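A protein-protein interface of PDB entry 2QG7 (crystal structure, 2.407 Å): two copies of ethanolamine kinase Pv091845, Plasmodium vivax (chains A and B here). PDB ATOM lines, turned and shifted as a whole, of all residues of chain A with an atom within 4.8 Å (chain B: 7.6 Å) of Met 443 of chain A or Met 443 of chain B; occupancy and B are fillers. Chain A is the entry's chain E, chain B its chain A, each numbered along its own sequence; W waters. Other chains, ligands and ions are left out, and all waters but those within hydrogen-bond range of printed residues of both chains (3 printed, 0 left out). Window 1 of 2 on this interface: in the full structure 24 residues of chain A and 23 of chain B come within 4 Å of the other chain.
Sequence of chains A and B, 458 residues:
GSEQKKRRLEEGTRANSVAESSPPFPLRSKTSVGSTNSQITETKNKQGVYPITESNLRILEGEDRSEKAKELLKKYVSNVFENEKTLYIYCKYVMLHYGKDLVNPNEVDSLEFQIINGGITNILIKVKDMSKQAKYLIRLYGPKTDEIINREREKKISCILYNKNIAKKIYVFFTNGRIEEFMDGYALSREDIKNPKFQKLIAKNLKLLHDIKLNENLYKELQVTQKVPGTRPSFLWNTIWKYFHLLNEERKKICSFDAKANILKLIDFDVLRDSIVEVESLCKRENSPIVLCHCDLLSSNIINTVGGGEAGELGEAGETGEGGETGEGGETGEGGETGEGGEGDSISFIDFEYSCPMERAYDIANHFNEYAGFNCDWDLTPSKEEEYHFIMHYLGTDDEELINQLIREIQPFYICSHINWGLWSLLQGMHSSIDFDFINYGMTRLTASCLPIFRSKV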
ATOM      1  N   ILE A 263       9.702  -9.928   7.463  1.00  0.00           N
ATOM      2  CA  ILE A 263       8.964 -10.836   6.549  1.00  0.00           C
ATOM      3  C   ILE A 263       7.590 -10.275   6.153  1.00  0.00           C
ATOM      4  O   ILE A 263       7.101 -10.509   5.045  1.00  0.00           O
ATOM      5  CB  ILE A 263       8.844 -12.288   7.150  1.00  0.00           C
ATOM      6  CG1 ILE A 263       8.326 -13.281   6.099  1.00  0.00           C
ATOM      7  CG2 ILE A 263       7.996 -12.302   8.462  1.00  0.00           C
ATOM      8  CD1 ILE A 263       9.081 -13.202   4.719  1.00  0.00           C
ATOM      9  N   ILE A 267       5.313  -8.811   2.075  1.00  0.00           N
ATOM     10  CA  ILE A 267       3.964  -9.166   1.667  1.00  0.00           C
ATOM     11  C   ILE A 267       3.182  -7.909   1.363  1.00  0.00           C
ATOM     12  O   ILE A 267       3.148  -6.994   2.191  1.00  0.00           O
ATOM     13  CB  ILE A 267       3.200 -10.006   2.767  1.00  0.00           C
ATOM     14  CG1 ILE A 267       3.963 -11.292   3.127  1.00  0.00           C
ATOM     15  CG2 ILE A 267       1.806 -10.393   2.253  1.00  0.00           C
ATOM     16  CD1 ILE A 267       3.662 -11.793   4.507  1.00  0.00           C
ATOM     17  N   LEU A 426       2.420 -16.659  11.091  1.00  0.00           N
ATOM     18  CA  LEU A 426       3.215 -15.448  11.056  1.00  0.00           C
ATOM     19  C   LEU A 426       3.114 -14.668  12.375  1.00  0.00           C
ATOM     20  O   LEU A 426       4.138 -14.146  12.861  1.00  0.00           O
ATOM     21  CB  LEU A 426       2.826 -14.567   9.862  1.00  0.00           C
ATOM     22  CG  LEU A 426       3.321 -15.027   8.493  1.00  0.00           C
ATOM     23  CD1 LEU A 426       2.793 -14.092   7.377  1.00  0.00           C
ATOM     24  CD2 LEU A 426       4.871 -15.138   8.408  1.00  0.00           C
ATOM     25  N   ILE A 439       7.632 -18.753  10.757  1.00  0.00           N
ATOM     26  CA  ILE A 439       7.722 -17.838   9.600  1.00  0.00           C
ATOM     27  C   ILE A 439       7.662 -18.578   8.263  1.00  0.00           C
ATOM     28  O   ILE A 439       6.920 -18.188   7.371  1.00  0.00           O
ATOM     29  CB  ILE A 439       9.033 -17.008   9.632  1.00  0.00           C
ATOM     30  CG1 ILE A 439       9.171 -16.247  10.966  1.00  0.00           C
ATOM     31  CG2 ILE A 439       9.165 -16.124   8.368  1.00  0.00           C
ATOM     32  CD1 ILE A 439       8.049 -15.266  11.286  1.00  0.00           C
ATOM     33  N   ASN A 440       8.479 -19.619   8.133  1.00  0.00           N
ATOM     34  CA  ASN A 440       8.551 -20.404   6.956  1.00  0.00           C
ATOM     35  C   ASN A 440       7.262 -21.204   6.740  1.00  0.00           C
ATOM     36  O   ASN A 440       6.807 -21.368   5.589  1.00  0.00           O
ATOM     37  CB  ASN A 440       9.748 -21.372   7.049  1.00  0.00           C
ATOM     38  CG  ASN A 440      11.053 -20.753   6.525  1.00  0.00           C
ATOM     39  OD1 ASN A 440      12.069 -20.698   7.231  1.00  0.00           O
ATOM     40  ND2 ASN A 440      11.019 -20.282   5.284  1.00  0.00           N
ATOM     41  N   TYR A 441       6.706 -21.729   7.841  1.00  0.00           N
ATOM     42  CA  TYR A 441       5.469 -22.469   7.754  1.00  0.00           C
ATOM     43  C   TYR A 441       4.353 -21.531   7.352  1.00  0.00           C
ATOM     44  O   TYR A 441       3.542 -21.917   6.532  1.00  0.00           O
ATOM     45  CB  TYR A 441       5.113 -23.197   9.066  1.00  0.00           C
ATOM     46  CG  TYR A 441       3.792 -23.924   9.000  1.00  0.00           C
ATOM     47  CD1 TYR A 441       3.683 -25.143   8.333  1.00  0.00           C
ATOM     48  CD2 TYR A 441       2.640 -23.387   9.597  1.00  0.00           C
ATOM     49  CE1 TYR A 441       2.482 -25.808   8.268  1.00  0.00           C
ATOM     50  CE2 TYR A 441       1.428 -24.056   9.523  1.00  0.00           C
ATOM     51  CZ  TYR A 441       1.359 -25.271   8.874  1.00  0.00           C
ATOM     52  OH  TYR A 441       0.143 -25.955   8.795  1.00  0.00           O
ATOM     53  N   GLY A 442       4.337 -20.329   7.921  1.00  0.00           N
ATOM     54  CA  GLY A 442       3.364 -19.267   7.588  1.00  0.00           C
ATOM     55  C   GLY A 442       3.384 -18.842   6.136  1.00  0.00           C
ATOM     56  O   GLY A 442       2.333 -18.661   5.499  1.00  0.00           O
ATOM     57  N   MET A 443       4.592 -18.708   5.591  1.00  0.00           N
ATOM     58  CA  MET A 443       4.836 -18.264   4.221  1.00  0.00           C
ATOM     59  C   MET A 443       4.512 -19.343   3.235  1.00  0.00           C
ATOM     60  O   MET A 443       4.040 -19.048   2.169  1.00  0.00           O
ATOM     61  CB  MET A 443       6.308 -17.812   4.033  1.00  0.00           C
ATOM     62  CG  MET A 443       6.658 -16.536   4.766  1.00  0.00           C
ATOM     63  SD  MET A 443       5.583 -15.146   4.260  1.00  0.00           S
ATOM     64  CE  MET A 443       6.054 -14.921   2.531  1.00  0.00           C
ATOM     65  N   THR A 444       4.797 -20.588   3.588  1.00  0.00           N
ATOM     66  CA  THR A 444       4.417 -21.736   2.797  1.00  0.00           C
ATOM     67  C   THR A 444       2.888 -21.888   2.668  1.00  0.00           C
ATOM     68  O   THR A 444       2.410 -22.182   1.560  1.00  0.00           O
ATOM     69  CB  THR A 444       5.013 -23.050   3.365  1.00  0.00           C
ATOM     70  OG1 THR A 444       6.423 -22.886   3.576  1.00  0.00           O
ATOM     71  CG2 THR A 444       4.775 -24.223   2.417  1.00  0.00           C
ATOM     72  N   ARG A 445       2.145 -21.688   3.773  1.00  0.00           N
ATOM     73  CA  ARG A 445       0.669 -21.694   3.730  1.00  0.00           C
ATOM     74  C   ARG A 445       0.131 -20.561   2.858  1.00  0.00           C
ATOM     75  O   ARG A 445      -0.757 -20.794   2.070  1.00  0.00           O
ATOM     76  CB  ARG A 445      -0.003 -21.625   5.122  1.00  0.00           C
ATOM     77  CG  ARG A 445       0.295 -22.745   6.067  1.00  0.00           C
ATOM     78  CD  ARG A 445       0.043 -24.116   5.474  1.00  0.00           C
ATOM     79  NE  ARG A 445      -1.370 -24.288   5.082  1.00  0.00           N
ATOM     80  CZ  ARG A 445      -2.337 -24.729   5.892  1.00  0.00           C
ATOM     81  NH1 ARG A 445      -3.549 -24.846   5.409  1.00  0.00           N
ATOM     82  NH2 ARG A 445      -2.102 -25.068   7.172  1.00  0.00           N
ATOM     83  N   LEU A 446       0.652 -19.345   3.035  1.00  0.00           N
ATOM     84  CA  LEU A 446       0.267 -18.197   2.223  1.00  0.00           C
ATOM     85  C   LEU A 446       0.592 -18.366   0.757  1.00  0.00           C
ATOM     86  O   LEU A 446      -0.160 -17.874  -0.065  1.00  0.00           O
ATOM     87  CB  LEU A 446       0.913 -16.914   2.716  1.00  0.00           C
ATOM     88  CG  LEU A 446       0.299 -16.294   3.986  1.00  0.00           C
ATOM     89  CD1 LEU A 446       0.959 -14.939   4.310  1.00  0.00           C
ATOM     90  CD2 LEU A 446      -1.252 -16.131   3.928  1.00  0.00           C
ATOM     91  N   THR A 447       1.706 -19.045   0.438  1.00  0.00           N
ATOM     92  CA  THR A 447       2.092 -19.392  -0.928  1.00  0.00           C
ATOM     93  C   THR A 447       1.043 -20.353  -1.517  1.00  0.00           C
ATOM     94  O   THR A 447       0.647 -20.211  -2.679  1.00  0.00           O
ATOM     95  CB  THR A 447       3.531 -20.043  -0.979  1.00  0.00           C
ATOM     96  OG1 THR A 447       4.509 -19.133  -0.460  1.00  0.00           O
ATOM     97  CG2 THR A 447       3.957 -20.398  -2.369  1.00  0.00           C
ATOM     98  N   ILE B 263       1.088 -15.505  -7.278  1.00  0.00           N
ATOM     99  CA  ILE B 263       2.085 -15.456  -6.211  1.00  0.00           C
ATOM    100  C   ILE B 263       2.940 -14.182  -6.232  1.00  0.00           C
ATOM    101  O   ILE B 263       3.219 -13.616  -5.164  1.00  0.00           O
ATOM    102  CB  ILE B 263       2.971 -16.733  -6.181  1.00  0.00           C
ATOM    103  CG1 ILE B 263       3.832 -16.755  -4.910  1.00  0.00           C
ATOM    104  CG2 ILE B 263       3.825 -16.804  -7.455  1.00  0.00           C
ATOM    105  CD1 ILE B 263       3.102 -16.637  -3.599  1.00  0.00           C
ATOM    106  N   LEU B 264       3.285 -13.704  -7.422  1.00  0.00           N
ATOM    107  CA  LEU B 264       3.987 -12.425  -7.551  1.00  0.00           C
ATOM    108  C   LEU B 264       3.189 -11.230  -7.042  1.00  0.00           C
ATOM    109  O   LEU B 264       3.763 -10.262  -6.578  1.00  0.00           O
ATOM    110  CB  LEU B 264       4.397 -12.164  -8.992  1.00  0.00           C
ATOM    111  CG  LEU B 264       5.164 -13.246  -9.725  1.00  0.00           C
ATOM    112  CD1 LEU B 264       5.366 -12.806 -11.183  1.00  0.00           C
ATOM    113  CD2 LEU B 264       6.456 -13.567  -9.018  1.00  0.00           C
ATOM    114  N   LEU B 266       1.155 -11.069  -4.489  1.00  0.00           N
ATOM    115  CA  LEU B 266       1.143 -11.041  -3.023  1.00  0.00           C
ATOM    116  C   LEU B 266       2.473 -10.486  -2.499  1.00  0.00           C
ATOM    117  O   LEU B 266       2.542  -9.953  -1.380  1.00  0.00           O
ATOM    118  CB  LEU B 266       0.863 -12.444  -2.444  1.00  0.00           C
ATOM    119  CG  LEU B 266       0.566 -12.519  -0.933  1.00  0.00           C
ATOM    120  CD1 LEU B 266      -0.710 -11.717  -0.487  1.00  0.00           C
ATOM    121  CD2 LEU B 266       0.457 -13.966  -0.461  1.00  0.00           C
ATOM    122  N   ILE B 267       3.528 -10.611  -3.309  1.00  0.00           N
ATOM    123  CA  ILE B 267       4.833 -10.018  -2.999  1.00  0.00           C
ATOM    124  C   ILE B 267       4.775  -8.517  -3.243  1.00  0.00           C
ATOM    125  O   ILE B 267       4.473  -8.099  -4.353  1.00  0.00           O
ATOM    126  CB  ILE B 267       5.967 -10.642  -3.826  1.00  0.00           C
ATOM    127  CG1 ILE B 267       6.017 -12.149  -3.624  1.00  0.00           C
ATOM    128  CG2 ILE B 267       7.303  -9.978  -3.478  1.00  0.00           C
ATOM    129  CD1 ILE B 267       6.755 -12.906  -4.747  1.00  0.00           C
ATOM    130  N   TRP B 421      18.515 -16.362  -6.042  1.00  0.00           N
ATOM    131  CA  TRP B 421      17.903 -17.645  -6.263  1.00  0.00           C
ATOM    132  C   TRP B 421      16.389 -17.669  -6.002  1.00  0.00           C
ATOM    133  O   TRP B 421      15.648 -18.437  -6.699  1.00  0.00           O
ATOM    134  CB  TRP B 421      18.639 -18.760  -5.528  1.00  0.00           C
ATOM    135  CG  TRP B 421      19.995 -19.024  -6.094  1.00  0.00           C
ATOM    136  CD1 TRP B 421      21.183 -18.753  -5.505  1.00  0.00           C
ATOM    137  CD2 TRP B 421      20.303 -19.589  -7.375  1.00  0.00           C
ATOM    138  NE1 TRP B 421      22.212 -19.126  -6.321  1.00  0.00           N
ATOM    139  CE2 TRP B 421      21.698 -19.635  -7.483  1.00  0.00           C
ATOM    140  CE3 TRP B 421      19.535 -20.101  -8.425  1.00  0.00           C
ATOM    141  CZ2 TRP B 421      22.351 -20.170  -8.616  1.00  0.00           C
ATOM    142  CZ3 TRP B 421      20.177 -20.602  -9.528  1.00  0.00           C
ATOM    143  CH2 TRP B 421      21.568 -20.626  -9.622  1.00  0.00           C
ATOM    144  N   GLY B 422      15.922 -16.813  -5.083  1.00  0.00           N
ATOM    145  CA  GLY B 422      14.478 -16.518  -4.942  1.00  0.00           C
ATOM    146  C   GLY B 422      13.786 -16.014  -6.187  1.00  0.00           C
ATOM    147  O   GLY B 422      12.740 -16.545  -6.579  1.00  0.00           O
ATOM    148  N   LEU B 423      14.351 -14.974  -6.799  1.00  0.00           N
ATOM    149  CA  LEU B 423      13.874 -14.389  -8.041  1.00  0.00           C
ATOM    150  C   LEU B 423      14.039 -15.313  -9.246  1.00  0.00           C
ATOM    151  O   LEU B 423      13.169 -15.392 -10.096  1.00  0.00           O
ATOM    152  CB  LEU B 423      14.614 -13.068  -8.301  1.00  0.00           C
ATOM    153  CG  LEU B 423      14.356 -11.890  -7.342  1.00  0.00           C
ATOM    154  CD1 LEU B 423      15.113 -10.664  -7.773  1.00  0.00           C
ATOM    155  CD2 LEU B 423      12.886 -11.537  -7.346  1.00  0.00           C
ATOM    156  N   SER B 425      14.078 -18.729  -9.193  1.00  0.00           N
ATOM    157  CA  SER B 425      13.142 -19.842  -8.993  1.00  0.00           C
ATOM    158  C   SER B 425      11.699 -19.448  -9.309  1.00  0.00           C
ATOM    159  O   SER B 425      11.004 -20.148 -10.055  1.00  0.00           O
ATOM    160  CB  SER B 425      13.271 -20.413  -7.567  1.00  0.00           C
ATOM    161  OG  SER B 425      12.687 -21.707  -7.507  1.00  0.00           O
ATOM    162  N   LEU B 426      11.277 -18.293  -8.784  1.00  0.00           N
ATOM    163  CA  LEU B 426      10.020 -17.723  -9.222  1.00  0.00           C
ATOM    164  C   LEU B 426       9.895 -17.527 -10.740  1.00  0.00           C
ATOM    165  O   LEU B 426       8.820 -17.792 -11.301  1.00  0.00           O
ATOM    166  CB  LEU B 426       9.765 -16.418  -8.505  1.00  0.00           C
ATOM    167  CG  LEU B 426       9.423 -16.481  -7.023  1.00  0.00           C
ATOM    168  CD1 LEU B 426       9.411 -15.049  -6.527  1.00  0.00           C
ATOM    169  CD2 LEU B 426       8.102 -17.187  -6.738  1.00  0.00           C
ATOM    170  N   ASP B 437       9.162 -27.957  -7.553  1.00  0.00           N
ATOM    171  CA  ASP B 437       8.357 -26.837  -7.085  1.00  0.00           C
ATOM    172  C   ASP B 437       9.164 -25.531  -7.010  1.00  0.00           C
ATOM    173  O   ASP B 437       9.742 -25.218  -5.971  1.00  0.00           O
ATOM    174  CB  ASP B 437       7.783 -27.149  -5.707  1.00  0.00           C
ATOM    175  CG  ASP B 437       6.570 -26.299  -5.388  1.00  0.00           C
ATOM    176  OD1 ASP B 437       5.888 -26.709  -4.404  1.00  0.00           O
ATOM    177  OD2 ASP B 437       6.267 -25.259  -6.081  1.00  0.00           O
ATOM    178  N   PHE B 438       9.169 -24.785  -8.112  1.00  0.00           N
ATOM    179  CA  PHE B 438       9.916 -23.555  -8.263  1.00  0.00           C
ATOM    180  C   PHE B 438       9.356 -22.433  -7.409  1.00  0.00           C
ATOM    181  O   PHE B 438      10.098 -21.652  -6.787  1.00  0.00           O
ATOM    182  CB  PHE B 438       9.962 -23.158  -9.741  1.00  0.00           C
ATOM    183  CG  PHE B 438      10.934 -23.976 -10.560  1.00  0.00           C
ATOM    184  CD1 PHE B 438      10.483 -24.789 -11.610  1.00  0.00           C
ATOM    185  CD2 PHE B 438      12.305 -23.943 -10.280  1.00  0.00           C
ATOM    186  CE1 PHE B 438      11.373 -25.552 -12.334  1.00  0.00           C
ATOM    187  CE2 PHE B 438      13.210 -24.700 -11.018  1.00  0.00           C
ATOM    188  CZ  PHE B 438      12.750 -25.512 -12.038  1.00  0.00           C
ATOM    189  N   ILE B 439       8.043 -22.371  -7.336  1.00  0.00           N
ATOM    190  CA  ILE B 439       7.369 -21.278  -6.619  1.00  0.00           C
ATOM    191  C   ILE B 439       7.635 -21.311  -5.127  1.00  0.00           C
ATOM    192  O   ILE B 439       7.926 -20.277  -4.524  1.00  0.00           O
ATOM    193  CB  ILE B 439       5.848 -21.248  -6.926  1.00  0.00           C
ATOM    194  CG1 ILE B 439       5.650 -20.925  -8.410  1.00  0.00           C
ATOM    195  CG2 ILE B 439       5.150 -20.200  -6.098  1.00  0.00           C
ATOM    196  CD1 ILE B 439       4.323 -21.391  -8.983  1.00  0.00           C
ATOM    197  N   ASN B 440       7.559 -22.503  -4.544  1.00  0.00           N
ATOM    198  CA  ASN B 440       7.786 -22.661  -3.143  1.00  0.00           C
ATOM    199  C   ASN B 440       9.231 -22.468  -2.760  1.00  0.00           C
ATOM    200  O   ASN B 440       9.526 -21.921  -1.688  1.00  0.00           O
ATOM    201  CB  ASN B 440       7.328 -24.046  -2.677  1.00  0.00           C
ATOM    202  CG  ASN B 440       5.979 -24.007  -2.042  1.00  0.00           C
ATOM    203  OD1 ASN B 440       5.732 -23.214  -1.109  1.00  0.00           O
ATOM    204  ND2 ASN B 440       5.064 -24.836  -2.565  1.00  0.00           N
ATOM    205  N   TYR B 441      10.122 -22.987  -3.597  1.00  0.00           N
ATOM    206  CA  TYR B 441      11.552 -22.788  -3.384  1.00  0.00           C
ATOM    207  C   TYR B 441      11.941 -21.293  -3.480  1.00  0.00           C
ATOM    208  O   TYR B 441      12.651 -20.796  -2.626  1.00  0.00           O
ATOM    209  CB  TYR B 441      12.379 -23.657  -4.329  1.00  0.00           C
ATOM    210  CG  TYR B 441      13.865 -23.563  -4.059  1.00  0.00           C
ATOM    211  CD1 TYR B 441      14.456 -24.322  -3.058  1.00  0.00           C
ATOM    212  CD2 TYR B 441      14.685 -22.725  -4.834  1.00  0.00           C
ATOM    213  CE1 TYR B 441      15.823 -24.224  -2.821  1.00  0.00           C
ATOM    214  CE2 TYR B 441      16.045 -22.612  -4.589  1.00  0.00           C
ATOM    215  CZ  TYR B 441      16.609 -23.352  -3.591  1.00  0.00           C
ATOM    216  OH  TYR B 441      17.961 -23.270  -3.374  1.00  0.00           O
ATOM    217  N   GLY B 442      11.427 -20.589  -4.490  1.00  0.00           N
ATOM    218  CA  GLY B 442      11.571 -19.132  -4.606  1.00  0.00           C
ATOM    219  C   GLY B 442      11.088 -18.347  -3.418  1.00  0.00           C
ATOM    220  O   GLY B 442      11.699 -17.378  -3.003  1.00  0.00           O
ATOM    221  N   MET B 443       9.968 -18.742  -2.855  1.00  0.00           N
ATOM    222  CA  MET B 443       9.404 -18.038  -1.708  1.00  0.00           C
ATOM    223  C   MET B 443      10.146 -18.378  -0.436  1.00  0.00           C
ATOM    224  O   MET B 443      10.250 -17.523   0.451  1.00  0.00           O
ATOM    225  CB  MET B 443       7.933 -18.386  -1.548  1.00  0.00           C
ATOM    226  CG  MET B 443       7.069 -17.843  -2.619  1.00  0.00           C
ATOM    227  SD  MET B 443       7.019 -16.057  -2.663  1.00  0.00           S
ATOM    228  CE  MET B 443       6.189 -15.616  -1.127  1.00  0.00           C
ATOM    229  N   THR B 444      10.675 -19.602  -0.348  1.00  0.00           N
ATOM    230  CA  THR B 444      11.520 -20.015   0.792  1.00  0.00           C
ATOM    231  C   THR B 444      12.856 -19.256   0.798  1.00  0.00           C
ATOM    232  O   THR B 444      13.361 -18.915   1.847  1.00  0.00           O
ATOM    233  CB  THR B 444      11.839 -21.521   0.742  1.00  0.00           C
ATOM    234  OG1 THR B 444      10.625 -22.233   0.603  1.00  0.00           O
ATOM    235  CG2 THR B 444      12.576 -22.034   1.973  1.00  0.00           C
ATOM    236  N   ARG B 445      13.430 -19.031  -0.388  1.00  0.00           N
ATOM    237  CA  ARG B 445      14.621 -18.180  -0.542  1.00  0.00           C
ATOM    238  C   ARG B 445      14.378 -16.691  -0.234  1.00  0.00           C
ATOM    239  O   ARG B 445      15.125 -16.097   0.540  1.00  0.00           O
ATOM    240  CB  ARG B 445      15.247 -18.388  -1.919  1.00  0.00           C
ATOM    241  CG  ARG B 445      15.752 -19.805  -2.198  1.00  0.00           C
ATOM    242  CD  ARG B 445      16.752 -20.329  -1.156  1.00  0.00           C
ATOM    243  NE  ARG B 445      18.033 -19.588  -1.081  1.00  0.00           N
ATOM    244  CZ  ARG B 445      19.124 -19.837  -1.818  1.00  0.00           C
ATOM    245  NH1 ARG B 445      20.224 -19.138  -1.615  1.00  0.00           N
ATOM    246  NH2 ARG B 445      19.144 -20.786  -2.766  1.00  0.00           N
ATOM    247  N   LEU B 446      13.356 -16.094  -0.832  1.00  0.00           N
ATOM    248  CA  LEU B 446      12.955 -14.747  -0.436  1.00  0.00           C
ATOM    249  C   LEU B 446      12.564 -14.562   1.007  1.00  0.00           C
ATOM    250  O   LEU B 446      12.735 -13.495   1.552  1.00  0.00           O
ATOM    251  CB  LEU B 446      11.798 -14.261  -1.303  1.00  0.00           C
ATOM    252  CG  LEU B 446      12.124 -13.963  -2.762  1.00  0.00           C
ATOM    253  CD1 LEU B 446      10.885 -13.500  -3.440  1.00  0.00           C
ATOM    254  CD2 LEU B 446      13.262 -12.890  -2.894  1.00  0.00           C
ATOM    255  N   THR B 447      11.962 -15.563   1.624  1.00  0.00           N
ATOM    256  CA  THR B 447      11.709 -15.519   3.063  1.00  0.00           C
ATOM    257  C   THR B 447      13.033 -15.452   3.810  1.00  0.00           C
ATOM    258  O   THR B 447      13.124 -14.690   4.771  1.00  0.00           O
ATOM    259  CB  THR B 447      10.907 -16.777   3.529  1.00  0.00           C
ATOM    260  OG1 THR B 447       9.639 -16.773   2.869  1.00  0.00           O
ATOM    261  CG2 THR B 447      10.672 -16.766   5.010  1.00  0.00           C
ATOM    262  N   ALA B 448      14.005 -16.311   3.417  1.00  0.00           N
ATOM    263  CA  ALA B 448      15.307 -16.394   4.049  1.00  0.00           C
ATOM    264  C   ALA B 448      16.075 -15.053   4.032  1.00  0.00           C
ATOM    265  O   ALA B 448      16.805 -14.700   4.976  1.00  0.00           O
ATOM    266  CB  ALA B 448      16.122 -17.475   3.383  1.00  0.00           C
ATOM    267  N   SER B 449      15.916 -14.321   2.939  1.00  0.00           N
ATOM    268  CA  SER B 449      16.447 -12.959   2.816  1.00  0.00           C
ATOM    269  C   SER B 449      15.915 -11.967   3.899  1.00  0.00           C
ATOM    270  O   SER B 449      16.540 -10.958   4.183  1.00  0.00           O
ATOM    271  CB  SER B 449      16.268 -12.438   1.391  1.00  0.00           C
ATOM    272  OG  SER B 449      14.935 -12.052   1.181  1.00  0.00           O
ATOM    273  N   LEU B 451      14.945 -13.160   7.069  1.00  0.00           N
ATOM    274  CA  LEU B 451      15.031 -13.863   8.350  1.00  0.00           C
ATOM    275  C   LEU B 451      16.148 -13.277   9.166  1.00  0.00           C
ATOM    276  O   LEU B 451      17.214 -13.056   8.620  1.00  0.00           O
ATOM    277  CB  LEU B 451      15.296 -15.362   8.145  1.00  0.00           C
ATOM    278  CG  LEU B 451      14.101 -16.255   7.767  1.00  0.00           C
ATOM    279  CD1 LEU B 451      14.540 -17.701   7.671  1.00  0.00           C
ATOM    280  CD2 LEU B 451      13.007 -16.145   8.786  1.00  0.00           C
HETATM  281  O   HOH W   1      13.349 -19.428   4.480  1.00  0.00           O
HETATM  282  O   HOH W   2       7.039 -21.423   0.523  1.00  0.00           O
HETATM  283  O   HOH W   3       3.048 -23.946  -0.491  1.00  0.00           O
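Met 443 of chain A touches just these residues of chain B: Met 443 (3.7 Å) and Thr 447 (3.5 Å). Met 443 of chain B touches just these residues of chain A: Met 443 (3.7 Å) and Thr 447 (3.6 Å). No residue of chain B comes within 4 Å of Gly 442 of chain A. Of the printed residues of chain B, Ile 439 of chain A touches Thr 447 and Leu 451. Printed residues of chain A within 4 Å of Leu 451 of chain B: Ile 439 (3.9 Å) and Asn 440 (3.9 Å). Gly 422 of chain B touches none of the printed residues of chain A. Leu 446 of chain B touches none of the printed residues of chain A. The nearest residue of chain B that does not touch Met 443 of chain A is Asn 440 of chain B (5.6 Å).
Hydrophobic or aromatic side chains of chain A within 4 Å of the printed part of chain B: Ile 263, Ile 267, Ile 439 and Met 443. Along chain A the printed residues that touch a printed residue of chain B span positions 263 to 447. Hydrophobic or aromatic side chains of chain B within 4 Å of the printed part of chain A: Ile 263, Leu 266, Ile 439, Met 443 and Leu 451. Among the printed residues, 14 pairs touch across the chains.
O of Met 443 of chain B sits at hydrogen-bond distance from OG1 of Thr 447 of chain B. OG1 of Thr 444 of chain B sits at hydrogen-bond distance from O of Asn 440 of chain B. ND2 of Asn 440 of chain B lies within hydrogen-bond range of OD1 of Asp 437 of chain B (2.8 Å). The backbone carbonyl oxygen (O) of Asn 440 of chain A sits at hydrogen-bond distance from the side-chain hydroxyl (OG1) of Thr 444 of chain A. The side-chain hydroxyl (OG1) of Thr 447 of chain A sits at hydrogen-bond distance from the backbone carbonyl oxygen (O) of Met 443 of chain A, 2.7 Å away.
Water W1 lies within hydrogen-bond range of ND2 of Asn 440 of chain A (2.6 Å), O of Thr 444 of chain B (2.7 Å) and N of Ala 448 of chain B (3.4 Å). Water W2 lies within hydrogen-bond range of OD1 of Asn 440 of chain B and OG1 of Thr 444 of chain A. Water W3 lies within hydrogen-bond range of O of Thr 444 of chain A and OD1 of Asn 440 of chain B.
Thr 447 of chain B touches Ile 439 of chain A (CG2 to CG2, 3.7 Å). Asn 440 of chain A touches Thr 447 of chain B (ND2 to CG2, 3.5 Å). OD1 of Asn 440 of chain A touches CD1 of Leu 451 of chain B, 3.9 Å away. CG of Met 443 of chain A touches OG1 of Thr 447 of chain B, at 3.5 Å. Thr 444 of chain A touches Asn 440 of chain B (CG2 to OD1, 3.8 Å). Leu 446 of chain A touches Leu 266 of chain B (O to CD2, 3.98 Å). Thr 447 of chain A touches Ile 263 of chain B. Ile 439 of chain B touches Thr 447 of chain A (CG2 to CG2, 3.9 Å). Asn 440 of chain B touches Thr 447 of chain A. OG1 of Thr 447 of chain A touches CG of Met 443 of chain B, at 3.6 Å.
Ile 439 of chain A touches Thr 447 of chain B, and with the chains exchanged Thr 447 of chain A touches Ile 439 of chain B. Asn 440 of chain A touches Thr 447 of chain B, and with the chains exchanged Thr 447 of chain A touches Asn 440 of chain B. Met 443 of chain B touches its own counterpart, Met 443 of chain A. Thr 444 of chain A touches Asn 440 of chain B, but with the chains exchanged Asn 440 of chain A does not touch Thr 444 of chain B (4.1 Å). Positions printed for both chains: 263, 267, 426, 439, 440, 441, 442, 443, 444, 445, 446 and 447. Of the 14 pairs that touch across the chains among the printed residues, 9 have their exchanged pair printed and touching as well.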
